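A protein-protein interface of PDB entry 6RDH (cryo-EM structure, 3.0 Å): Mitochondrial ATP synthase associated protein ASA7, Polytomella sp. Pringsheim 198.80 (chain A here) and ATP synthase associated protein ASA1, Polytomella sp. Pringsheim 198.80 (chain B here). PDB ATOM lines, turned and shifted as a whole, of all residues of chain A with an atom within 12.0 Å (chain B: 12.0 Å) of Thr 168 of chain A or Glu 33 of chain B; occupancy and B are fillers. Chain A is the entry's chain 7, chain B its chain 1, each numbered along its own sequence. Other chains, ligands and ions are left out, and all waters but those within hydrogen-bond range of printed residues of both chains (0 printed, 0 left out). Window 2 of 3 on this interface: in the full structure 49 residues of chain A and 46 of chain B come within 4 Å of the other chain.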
ATOM      1  N   ASN A 160     -22.500  20.701  20.077  1.00  0.00           N
ATOM      2  CA  ASN A 160     -21.748  20.626  18.826  1.00  0.00           C
ATOM      3  C   ASN A 160     -22.382  21.485  17.741  1.00  0.00           C
ATOM      4  O   ASN A 160     -21.672  22.140  16.966  1.00  0.00           O
ATOM      5  CB  ASN A 160     -21.643  19.179  18.362  1.00  0.00           C
ATOM      6  CG  ASN A 160     -20.603  18.400  19.131  1.00  0.00           C
ATOM      7  OD1 ASN A 160     -19.761  18.975  19.813  1.00  0.00           O
ATOM      8  ND2 ASN A 160     -20.641  17.082  19.005  1.00  0.00           N
ATOM      9  N   TYR A 161     -23.713  21.502  17.686  1.00  0.00           N
ATOM     10  CA  TYR A 161     -24.418  22.385  16.767  1.00  0.00           C
ATOM     11  C   TYR A 161     -24.164  23.842  17.107  1.00  0.00           C
ATOM     12  O   TYR A 161     -23.932  24.661  16.216  1.00  0.00           O
ATOM     13  CB  TYR A 161     -25.916  22.097  16.805  1.00  0.00           C
ATOM     14  CG  TYR A 161     -26.749  23.180  16.176  1.00  0.00           C
ATOM     15  CD1 TYR A 161     -27.478  24.062  16.950  1.00  0.00           C
ATOM     16  CD2 TYR A 161     -26.813  23.314  14.803  1.00  0.00           C
ATOM     17  CE1 TYR A 161     -28.219  25.051  16.377  1.00  0.00           C
ATOM     18  CE2 TYR A 161     -27.563  24.296  14.225  1.00  0.00           C
ATOM     19  CZ  TYR A 161     -28.268  25.159  15.021  1.00  0.00           C
ATOM     20  OH  TYR A 161     -29.031  26.151  14.467  1.00  0.00           O
ATOM     21  N   ALA A 162     -24.199  24.182  18.390  1.00  0.00           N
ATOM     22  CA  ALA A 162     -24.019  25.567  18.791  1.00  0.00           C
ATOM     23  C   ALA A 162     -22.578  26.015  18.635  1.00  0.00           C
ATOM     24  O   ALA A 162     -22.315  27.215  18.558  1.00  0.00           O
ATOM     25  CB  ALA A 162     -24.480  25.762  20.229  1.00  0.00           C
ATOM     26  N   ALA A 163     -21.634  25.078  18.610  1.00  0.00           N
ATOM     27  CA  ALA A 163     -20.264  25.422  18.269  1.00  0.00           C
ATOM     28  C   ALA A 163     -20.054  25.537  16.773  1.00  0.00           C
ATOM     29  O   ALA A 163     -19.130  26.229  16.344  1.00  0.00           O
ATOM     30  CB  ALA A 163     -19.301  24.389  18.836  1.00  0.00           C
ATOM     31  N   ARG A 164     -20.876  24.869  15.969  1.00  0.00           N
ATOM     32  CA  ARG A 164     -20.799  25.088  14.530  1.00  0.00           C
ATOM     33  C   ARG A 164     -21.372  26.430  14.120  1.00  0.00           C
ATOM     34  O   ARG A 164     -21.044  26.917  13.037  1.00  0.00           O
ATOM     35  CB  ARG A 164     -21.525  23.977  13.786  1.00  0.00           C
ATOM     36  CG  ARG A 164     -20.695  22.733  13.628  1.00  0.00           C
ATOM     37  CD  ARG A 164     -21.399  21.703  12.788  1.00  0.00           C
ATOM     38  NE  ARG A 164     -21.792  22.239  11.495  1.00  0.00           N
ATOM     39  CZ  ARG A 164     -21.001  22.250  10.430  1.00  0.00           C
ATOM     40  NH1 ARG A 164     -21.437  22.752   9.290  1.00  0.00           N
ATOM     41  NH2 ARG A 164     -19.774  21.763  10.508  1.00  0.00           N
ATOM     42  N   ARG A 165     -22.221  27.035  14.946  1.00  0.00           N
ATOM     43  CA  ARG A 165     -22.803  28.331  14.636  1.00  0.00           C
ATOM     44  C   ARG A 165     -22.027  29.482  15.239  1.00  0.00           C
ATOM     45  O   ARG A 165     -22.399  30.637  15.027  1.00  0.00           O
ATOM     46  CB  ARG A 165     -24.251  28.395  15.102  1.00  0.00           C
ATOM     47  CG  ARG A 165     -25.144  27.353  14.491  1.00  0.00           C
ATOM     48  CD  ARG A 165     -25.531  27.670  13.078  1.00  0.00           C
ATOM     49  NE  ARG A 165     -24.598  27.094  12.129  1.00  0.00           N
ATOM     50  CZ  ARG A 165     -24.878  26.836  10.862  1.00  0.00           C
ATOM     51  NH1 ARG A 165     -23.951  26.314  10.075  1.00  0.00           N
ATOM     52  NH2 ARG A 165     -26.085  27.084  10.380  1.00  0.00           N
ATOM     53  N   ARG A 166     -20.975  29.201  15.995  1.00  0.00           N
ATOM     54  CA  ARG A 166     -20.009  30.221  16.378  1.00  0.00           C
ATOM     55  C   ARG A 166     -18.872  30.238  15.368  1.00  0.00           C
ATOM     56  O   ARG A 166     -17.713  30.037  15.689  1.00  0.00           O
ATOM     57  CB  ARG A 166     -19.482  29.968  17.781  1.00  0.00           C
ATOM     58  CG  ARG A 166     -20.364  30.478  18.874  1.00  0.00           C
ATOM     59  CD  ARG A 166     -19.635  30.405  20.184  1.00  0.00           C
ATOM     60  NE  ARG A 166     -19.065  29.083  20.388  1.00  0.00           N
ATOM     61  CZ  ARG A 166     -19.697  28.091  20.997  1.00  0.00           C
ATOM     62  NH1 ARG A 166     -19.107  26.918  21.142  1.00  0.00           N
ATOM     63  NH2 ARG A 166     -20.920  28.272  21.460  1.00  0.00           N
ATOM     64  N   SER A 167     -19.237  30.461  14.120  1.00  0.00           N
ATOM     65  CA  SER A 167     -18.254  30.471  13.059  1.00  0.00           C
ATOM     66  C   SER A 167     -17.619  31.844  12.976  1.00  0.00           C
ATOM     67  O   SER A 167     -18.245  32.860  13.279  1.00  0.00           O
ATOM     68  CB  SER A 167     -18.888  30.095  11.726  1.00  0.00           C
ATOM     69  OG  SER A 167     -17.930  30.111  10.691  1.00  0.00           O
ATOM     70  N   THR A 168     -16.354  31.865  12.588  1.00  0.00           N
ATOM     71  CA  THR A 168     -15.636  33.113  12.427  1.00  0.00           C
ATOM     72  C   THR A 168     -16.077  33.886  11.195  1.00  0.00           C
ATOM     73  O   THR A 168     -15.779  35.078  11.094  1.00  0.00           O
ATOM     74  CB  THR A 168     -14.141  32.837  12.355  1.00  0.00           C
ATOM     75  OG1 THR A 168     -13.868  32.015  11.215  1.00  0.00           O
ATOM     76  CG2 THR A 168     -13.691  32.111  13.594  1.00  0.00           C
ATOM     77  N   VAL A 169     -16.772  33.240  10.264  1.00  0.00           N
ATOM     78  CA  VAL A 169     -17.285  33.915   9.084  1.00  0.00           C
ATOM     79  C   VAL A 169     -18.686  34.434   9.355  1.00  0.00           C
ATOM     80  O   VAL A 169     -18.899  35.642   9.434  1.00  0.00           O
ATOM     81  CB  VAL A 169     -17.283  32.969   7.878  1.00  0.00           C
ATOM     82  CG1 VAL A 169     -17.825  33.669   6.671  1.00  0.00           C
ATOM     83  CG2 VAL A 169     -15.894  32.473   7.622  1.00  0.00           C
ATOM     84  N   HIS A 170     -19.639  33.534   9.564  1.00  0.00           N
ATOM     85  CA  HIS A 170     -21.031  33.924   9.719  1.00  0.00           C
ATOM     86  C   HIS A 170     -21.769  32.775  10.375  1.00  0.00           C
ATOM     87  O   HIS A 170     -21.385  31.618  10.182  1.00  0.00           O
ATOM     88  CB  HIS A 170     -21.662  34.264   8.362  1.00  0.00           C
ATOM     89  CG  HIS A 170     -22.908  35.084   8.457  1.00  0.00           C
ATOM     90  ND1 HIS A 170     -22.895  36.458   8.528  1.00  0.00           N
ATOM     91  CD2 HIS A 170     -24.209  34.723   8.494  1.00  0.00           C
ATOM     92  CE1 HIS A 170     -24.135  36.904   8.607  1.00  0.00           C
ATOM     93  NE2 HIS A 170     -24.951  35.871   8.587  1.00  0.00           N
ATOM     94  N   PRO A 171     -22.806  33.051  11.169  1.00  0.00           N
ATOM     95  CA  PRO A 171     -23.635  31.958  11.693  1.00  0.00           C
ATOM     96  C   PRO A 171     -24.384  31.188  10.630  1.00  0.00           C
ATOM     97  O   PRO A 171     -24.673  30.006  10.829  1.00  0.00           O
ATOM     98  CB  PRO A 171     -24.609  32.682  12.625  1.00  0.00           C
ATOM     99  CG  PRO A 171     -23.941  33.917  12.984  1.00  0.00           C
ATOM    100  CD  PRO A 171     -23.090  34.321  11.847  1.00  0.00           C
ATOM    101  N   ALA A 172     -24.711  31.815   9.508  1.00  0.00           N
ATOM    102  CA  ALA A 172     -25.528  31.207   8.472  1.00  0.00           C
ATOM    103  C   ALA A 172     -24.721  30.747   7.274  1.00  0.00           C
ATOM    104  O   ALA A 172     -25.310  30.407   6.246  1.00  0.00           O
ATOM    105  CB  ALA A 172     -26.602  32.183   8.005  1.00  0.00           C
ATOM    106  N   ILE A 173     -23.409  30.734   7.370  1.00  0.00           N
ATOM    107  CA  ILE A 173     -22.584  30.386   6.224  1.00  0.00           C
ATOM    108  C   ILE A 173     -22.608  28.878   6.034  1.00  0.00           C
ATOM    109  O   ILE A 173     -22.820  28.110   6.977  1.00  0.00           O
ATOM    110  CB  ILE A 173     -21.152  30.944   6.397  1.00  0.00           C
ATOM    111  CG1 ILE A 173     -20.439  31.065   5.056  1.00  0.00           C
ATOM    112  CG2 ILE A 173     -20.324  30.109   7.355  1.00  0.00           C
ATOM    113  CD1 ILE A 173     -21.208  31.804   4.020  1.00  0.00           C
ATOM    114  N   GLY A 174     -22.461  28.451   4.790  1.00  0.00           N
ATOM    115  CA  GLY A 174     -22.439  27.042   4.486  1.00  0.00           C
ATOM    116  C   GLY A 174     -21.494  26.763   3.348  1.00  0.00           C
ATOM    117  O   GLY A 174     -20.714  27.636   2.973  1.00  0.00           O
ATOM    118  N   SER A 175     -21.550  25.562   2.780  1.00  0.00           N
ATOM    119  CA  SER A 175     -20.628  25.232   1.705  1.00  0.00           C
ATOM    120  C   SER A 175     -21.085  25.767   0.360  1.00  0.00           C
ATOM    121  O   SER A 175     -20.240  26.094  -0.474  1.00  0.00           O
ATOM    122  CB  SER A 175     -20.422  23.727   1.623  1.00  0.00           C
ATOM    123  OG  SER A 175     -19.684  23.271   2.736  1.00  0.00           O
ATOM    124  N   ALA A 178     -20.291  29.589   0.252  1.00  0.00           N
ATOM    125  CA  ALA A 178     -18.849  29.795   0.222  1.00  0.00           C
ATOM    126  C   ALA A 178     -18.242  29.333  -1.095  1.00  0.00           C
ATOM    127  O   ALA A 178     -17.301  29.961  -1.589  1.00  0.00           O
ATOM    128  CB  ALA A 178     -18.187  29.083   1.393  1.00  0.00           C
ATOM    129  N   ARG B  28     -19.272  25.281  26.163  1.00  0.00           N
ATOM    130  CA  ARG B  28     -18.083  25.381  25.338  1.00  0.00           C
ATOM    131  C   ARG B  28     -17.918  26.811  24.853  1.00  0.00           C
ATOM    132  O   ARG B  28     -18.898  27.527  24.641  1.00  0.00           O
ATOM    133  CB  ARG B  28     -18.170  24.447  24.141  1.00  0.00           C
ATOM    134  CG  ARG B  28     -18.383  23.005  24.511  1.00  0.00           C
ATOM    135  CD  ARG B  28     -18.652  22.178  23.288  1.00  0.00           C
ATOM    136  NE  ARG B  28     -17.763  22.556  22.204  1.00  0.00           N
ATOM    137  CZ  ARG B  28     -17.742  21.952  21.027  1.00  0.00           C
ATOM    138  NH1 ARG B  28     -16.905  22.359  20.088  1.00  0.00           N
ATOM    139  NH2 ARG B  28     -18.557  20.935  20.801  1.00  0.00           N
ATOM    140  N   SER B  29     -16.667  27.240  24.710  1.00  0.00           N
ATOM    141  CA  SER B  29     -16.356  28.539  24.127  1.00  0.00           C
ATOM    142  C   SER B  29     -15.260  28.315  23.096  1.00  0.00           C
ATOM    143  O   SER B  29     -14.079  28.526  23.364  1.00  0.00           O
ATOM    144  CB  SER B  29     -15.916  29.531  25.191  1.00  0.00           C
ATOM    145  OG  SER B  29     -14.680  29.134  25.759  1.00  0.00           O
ATOM    146  N   ASP B  30     -15.657  27.913  21.896  1.00  0.00           N
ATOM    147  CA  ASP B  30     -14.704  27.724  20.820  1.00  0.00           C
ATOM    148  C   ASP B  30     -15.407  28.007  19.508  1.00  0.00           C
ATOM    149  O   ASP B  30     -16.633  27.934  19.409  1.00  0.00           O
ATOM    150  CB  ASP B  30     -14.090  26.321  20.824  1.00  0.00           C
ATOM    151  CG  ASP B  30     -15.116  25.231  20.641  1.00  0.00           C
ATOM    152  OD1 ASP B  30     -16.259  25.420  21.084  1.00  0.00           O
ATOM    153  OD2 ASP B  30     -14.784  24.181  20.057  1.00  0.00           O
ATOM    154  N   PHE B  31     -14.611  28.334  18.504  1.00  0.00           N
ATOM    155  CA  PHE B  31     -15.100  28.813  17.228  1.00  0.00           C
ATOM    156  C   PHE B  31     -14.832  27.777  16.151  1.00  0.00           C
ATOM    157  O   PHE B  31     -13.970  26.909  16.296  1.00  0.00           O
ATOM    158  CB  PHE B  31     -14.441  30.140  16.861  1.00  0.00           C
ATOM    159  CG  PHE B  31     -14.890  31.291  17.706  1.00  0.00           C
ATOM    160  CD1 PHE B  31     -15.846  32.165  17.245  1.00  0.00           C
ATOM    161  CD2 PHE B  31     -14.350  31.503  18.960  1.00  0.00           C
ATOM    162  CE1 PHE B  31     -16.260  33.217  18.018  1.00  0.00           C
ATOM    163  CE2 PHE B  31     -14.765  32.556  19.737  1.00  0.00           C
ATOM    164  CZ  PHE B  31     -15.715  33.411  19.265  1.00  0.00           C
ATOM    165  N   THR B  32     -15.590  27.871  15.065  1.00  0.00           N
ATOM    166  CA  THR B  32     -15.446  26.973  13.928  1.00  0.00           C
ATOM    167  C   THR B  32     -14.765  27.737  12.804  1.00  0.00           C
ATOM    168  O   THR B  32     -15.415  28.483  12.070  1.00  0.00           O
ATOM    169  CB  THR B  32     -16.799  26.434  13.485  1.00  0.00           C
ATOM    170  OG1 THR B  32     -17.496  25.925  14.622  1.00  0.00           O
ATOM    171  CG2 THR B  32     -16.617  25.319  12.501  1.00  0.00           C
ATOM    172  N   GLU B  33     -13.456  27.543  12.663  1.00  0.00           N
ATOM    173  CA  GLU B  33     -12.686  28.303  11.693  1.00  0.00           C
ATOM    174  C   GLU B  33     -12.803  27.773  10.274  1.00  0.00           C
ATOM    175  O   GLU B  33     -12.426  28.479   9.336  1.00  0.00           O
ATOM    176  CB  GLU B  33     -11.213  28.334  12.097  1.00  0.00           C
ATOM    177  CG  GLU B  33     -10.923  29.197  13.304  1.00  0.00           C
ATOM    178  CD  GLU B  33     -10.810  28.394  14.575  1.00  0.00           C
ATOM    179  OE1 GLU B  33     -10.991  27.161  14.512  1.00  0.00           O
ATOM    180  OE2 GLU B  33     -10.535  28.992  15.636  1.00  0.00           O
ATOM    181  N   GLU B  34     -13.299  26.561  10.091  1.00  0.00           N
ATOM    182  CA  GLU B  34     -13.469  26.008   8.758  1.00  0.00           C
ATOM    183  C   GLU B  34     -14.930  26.066   8.346  1.00  0.00           C
ATOM    184  O   GLU B  34     -15.821  26.282   9.164  1.00  0.00           O
ATOM    185  CB  GLU B  34     -12.968  24.567   8.701  1.00  0.00           C
ATOM    186  CG  GLU B  34     -13.705  23.605   9.620  1.00  0.00           C
ATOM    187  CD  GLU B  34     -13.094  23.505  11.009  1.00  0.00           C
ATOM    188  OE1 GLU B  34     -12.177  24.295  11.322  1.00  0.00           O
ATOM    189  OE2 GLU B  34     -13.537  22.639  11.792  1.00  0.00           O
ATOM    190  N   ILE B  35     -15.174  25.882   7.059  1.00  0.00           N
ATOM    191  CA  ILE B  35     -16.525  25.728   6.543  1.00  0.00           C
ATOM    192  C   ILE B  35     -16.614  24.338   5.942  1.00  0.00           C
ATOM    193  O   ILE B  35     -16.006  24.061   4.903  1.00  0.00           O
ATOM    194  CB  ILE B  35     -16.892  26.801   5.518  1.00  0.00           C
ATOM    195  CG1 ILE B  35     -16.901  28.168   6.178  1.00  0.00           C
ATOM    196  CG2 ILE B  35     -18.250  26.515   4.934  1.00  0.00           C
ATOM    197  CD1 ILE B  35     -17.181  29.276   5.228  1.00  0.00           C
ATOM    198  N   THR B  36     -17.367  23.464   6.599  1.00  0.00           N
ATOM    199  CA  THR B  36     -17.428  22.056   6.257  1.00  0.00           C
ATOM    200  C   THR B  36     -18.897  21.664   6.134  1.00  0.00           C
ATOM    201  O   THR B  36     -19.765  22.243   6.788  1.00  0.00           O
ATOM    202  CB  THR B  36     -16.694  21.235   7.339  1.00  0.00           C
ATOM    203  OG1 THR B  36     -15.340  21.685   7.422  1.00  0.00           O
ATOM    204  CG2 THR B  36     -16.625  19.758   7.007  1.00  0.00           C
ATOM    205  N   ALA B  37     -19.177  20.722   5.232  1.00  0.00           N
ATOM    206  CA  ALA B  37     -20.464  20.052   5.192  1.00  0.00           C
ATOM    207  C   ALA B  37     -20.715  19.348   6.527  1.00  0.00           C
ATOM    208  O   ALA B  37     -19.785  18.825   7.143  1.00  0.00           O
ATOM    209  CB  ALA B  37     -20.489  19.049   4.042  1.00  0.00           C
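The guanidinium group (NH2) of Arg 28 of chain B sits at hydrogen-bond distance from the side-chain amide oxygen (OD1) of Asn 160 of chain A (2.5 Å). The guanidinium group of Arg 166 of chain A is in salt-bridge range of the side-chain carboxylate of Asp 30 of chain B (3.2 Å). O of Arg 166 of chain A lies within hydrogen-bond range of N of Thr 32 of chain B (3.1 Å). The side-chain hydroxyl of Ser 167 of chain A is in hydrogen-bond range of the backbone carbonyl oxygen of Thr 32 of chain B (3.3 Å). NH1 of Arg 164 of chain A sits at hydrogen-bond distance from O of Thr 36 of chain B, 3.1 Å away. The backbone carbonyl oxygen of Ala 163 of chain A sits close to the side-chain hydroxyl of Thr 32 of chain B (2.4 Å).
The guanidinium group (NH1) of Arg 28 of chain B is in salt-bridge range of the side-chain carboxylate (OD2) of Asp 30 of chain B. The guanidinium group (NH2) of Arg 166 of chain A is in hydrogen-bond range of the backbone carbonyl oxygen (O) of Ala 162 of chain A, at 3.4 Å. The backbone NH of Val 169 of chain A sits close to the side-chain hydroxyl of Ser 167 of chain A (3.4 Å).
Among the printed residues, pairs that only touch across the chains: Arg 166 of chain A with Phe 31 of chain B (3.2 Å), Gly 174 of chain A with Ile 35 of chain B (3.3 Å), Ala 163 of chain A with Arg 28 of chain B (3.4 Å), Arg 164 of chain A with Thr 32 of chain B (3.4 Å), Thr 168 of chain A with Thr 32 of chain B (3.5 Å), Arg 166 of chain A with Arg 28 of chain B (3.6 Å), Ser 175 of chain A with Ala 37 of chain B (3.6 Å), Ile 173 of chain A with Ile 35 of chain B (3.7 Å), Ser 175 of chain A with Thr 36 of chain B (3.8 Å), Thr 168 of chain A with Phe 31 of chain B (3.9 Å), Ala 163 of chain A with Asp 30 of chain B (3.9 Å), Thr 168 of chain A with Glu 33 of chain B (3.9 Å) and Ala 178 of chain A with Ile 35 of chain B (3.97 Å).
Of chain B, only Thr 32 comes within 4 Å of Ser 167 of chain A. Thr 168 of chain A touches three residues of chain B. No residue of chain B comes within 4 Å of Val 169 of chain A. Of the printed residues of chain B, Gly 174 of chain A touches Ile 35 (3.3 Å). Printed residues of chain A within 4 Å of Arg 28 of chain B: Asn 160, Ala 163 and Arg 166. Phe 31 of chain B touches just these residues of chain A: Arg 166 and Thr 168. Printed residues of chain A within 4 Å of Thr 32 of chain B: Ala 163, Arg 164, Arg 166, Ser 167 and Thr 168. Of chain A, only Thr 168 (3.9 Å) comes within 4 Å of Glu 33 of chain B. Of the printed residues of chain A, Ala 37 of chain B touches Ser 175. The nearest residue of chain A that does not touch Glu 33 of chain B is Ser 167 of chain A (5.5 Å). The nearest printed residue of chain B that does not touch Arg 164 of chain A is Ala 37 of chain B (4.4 Å).
Of the 17 printed residues of chain A, 10 touch a printed residue of chain B. Hydrophobic or aromatic side chains of chain A that line the printed part of chain B: Ala 163, Ile 173 and Ala 178. Of the 10 printed residues of chain B, 8 touch a printed residue of chain A. Among the printed residues, 19 pairs touch across the chains.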
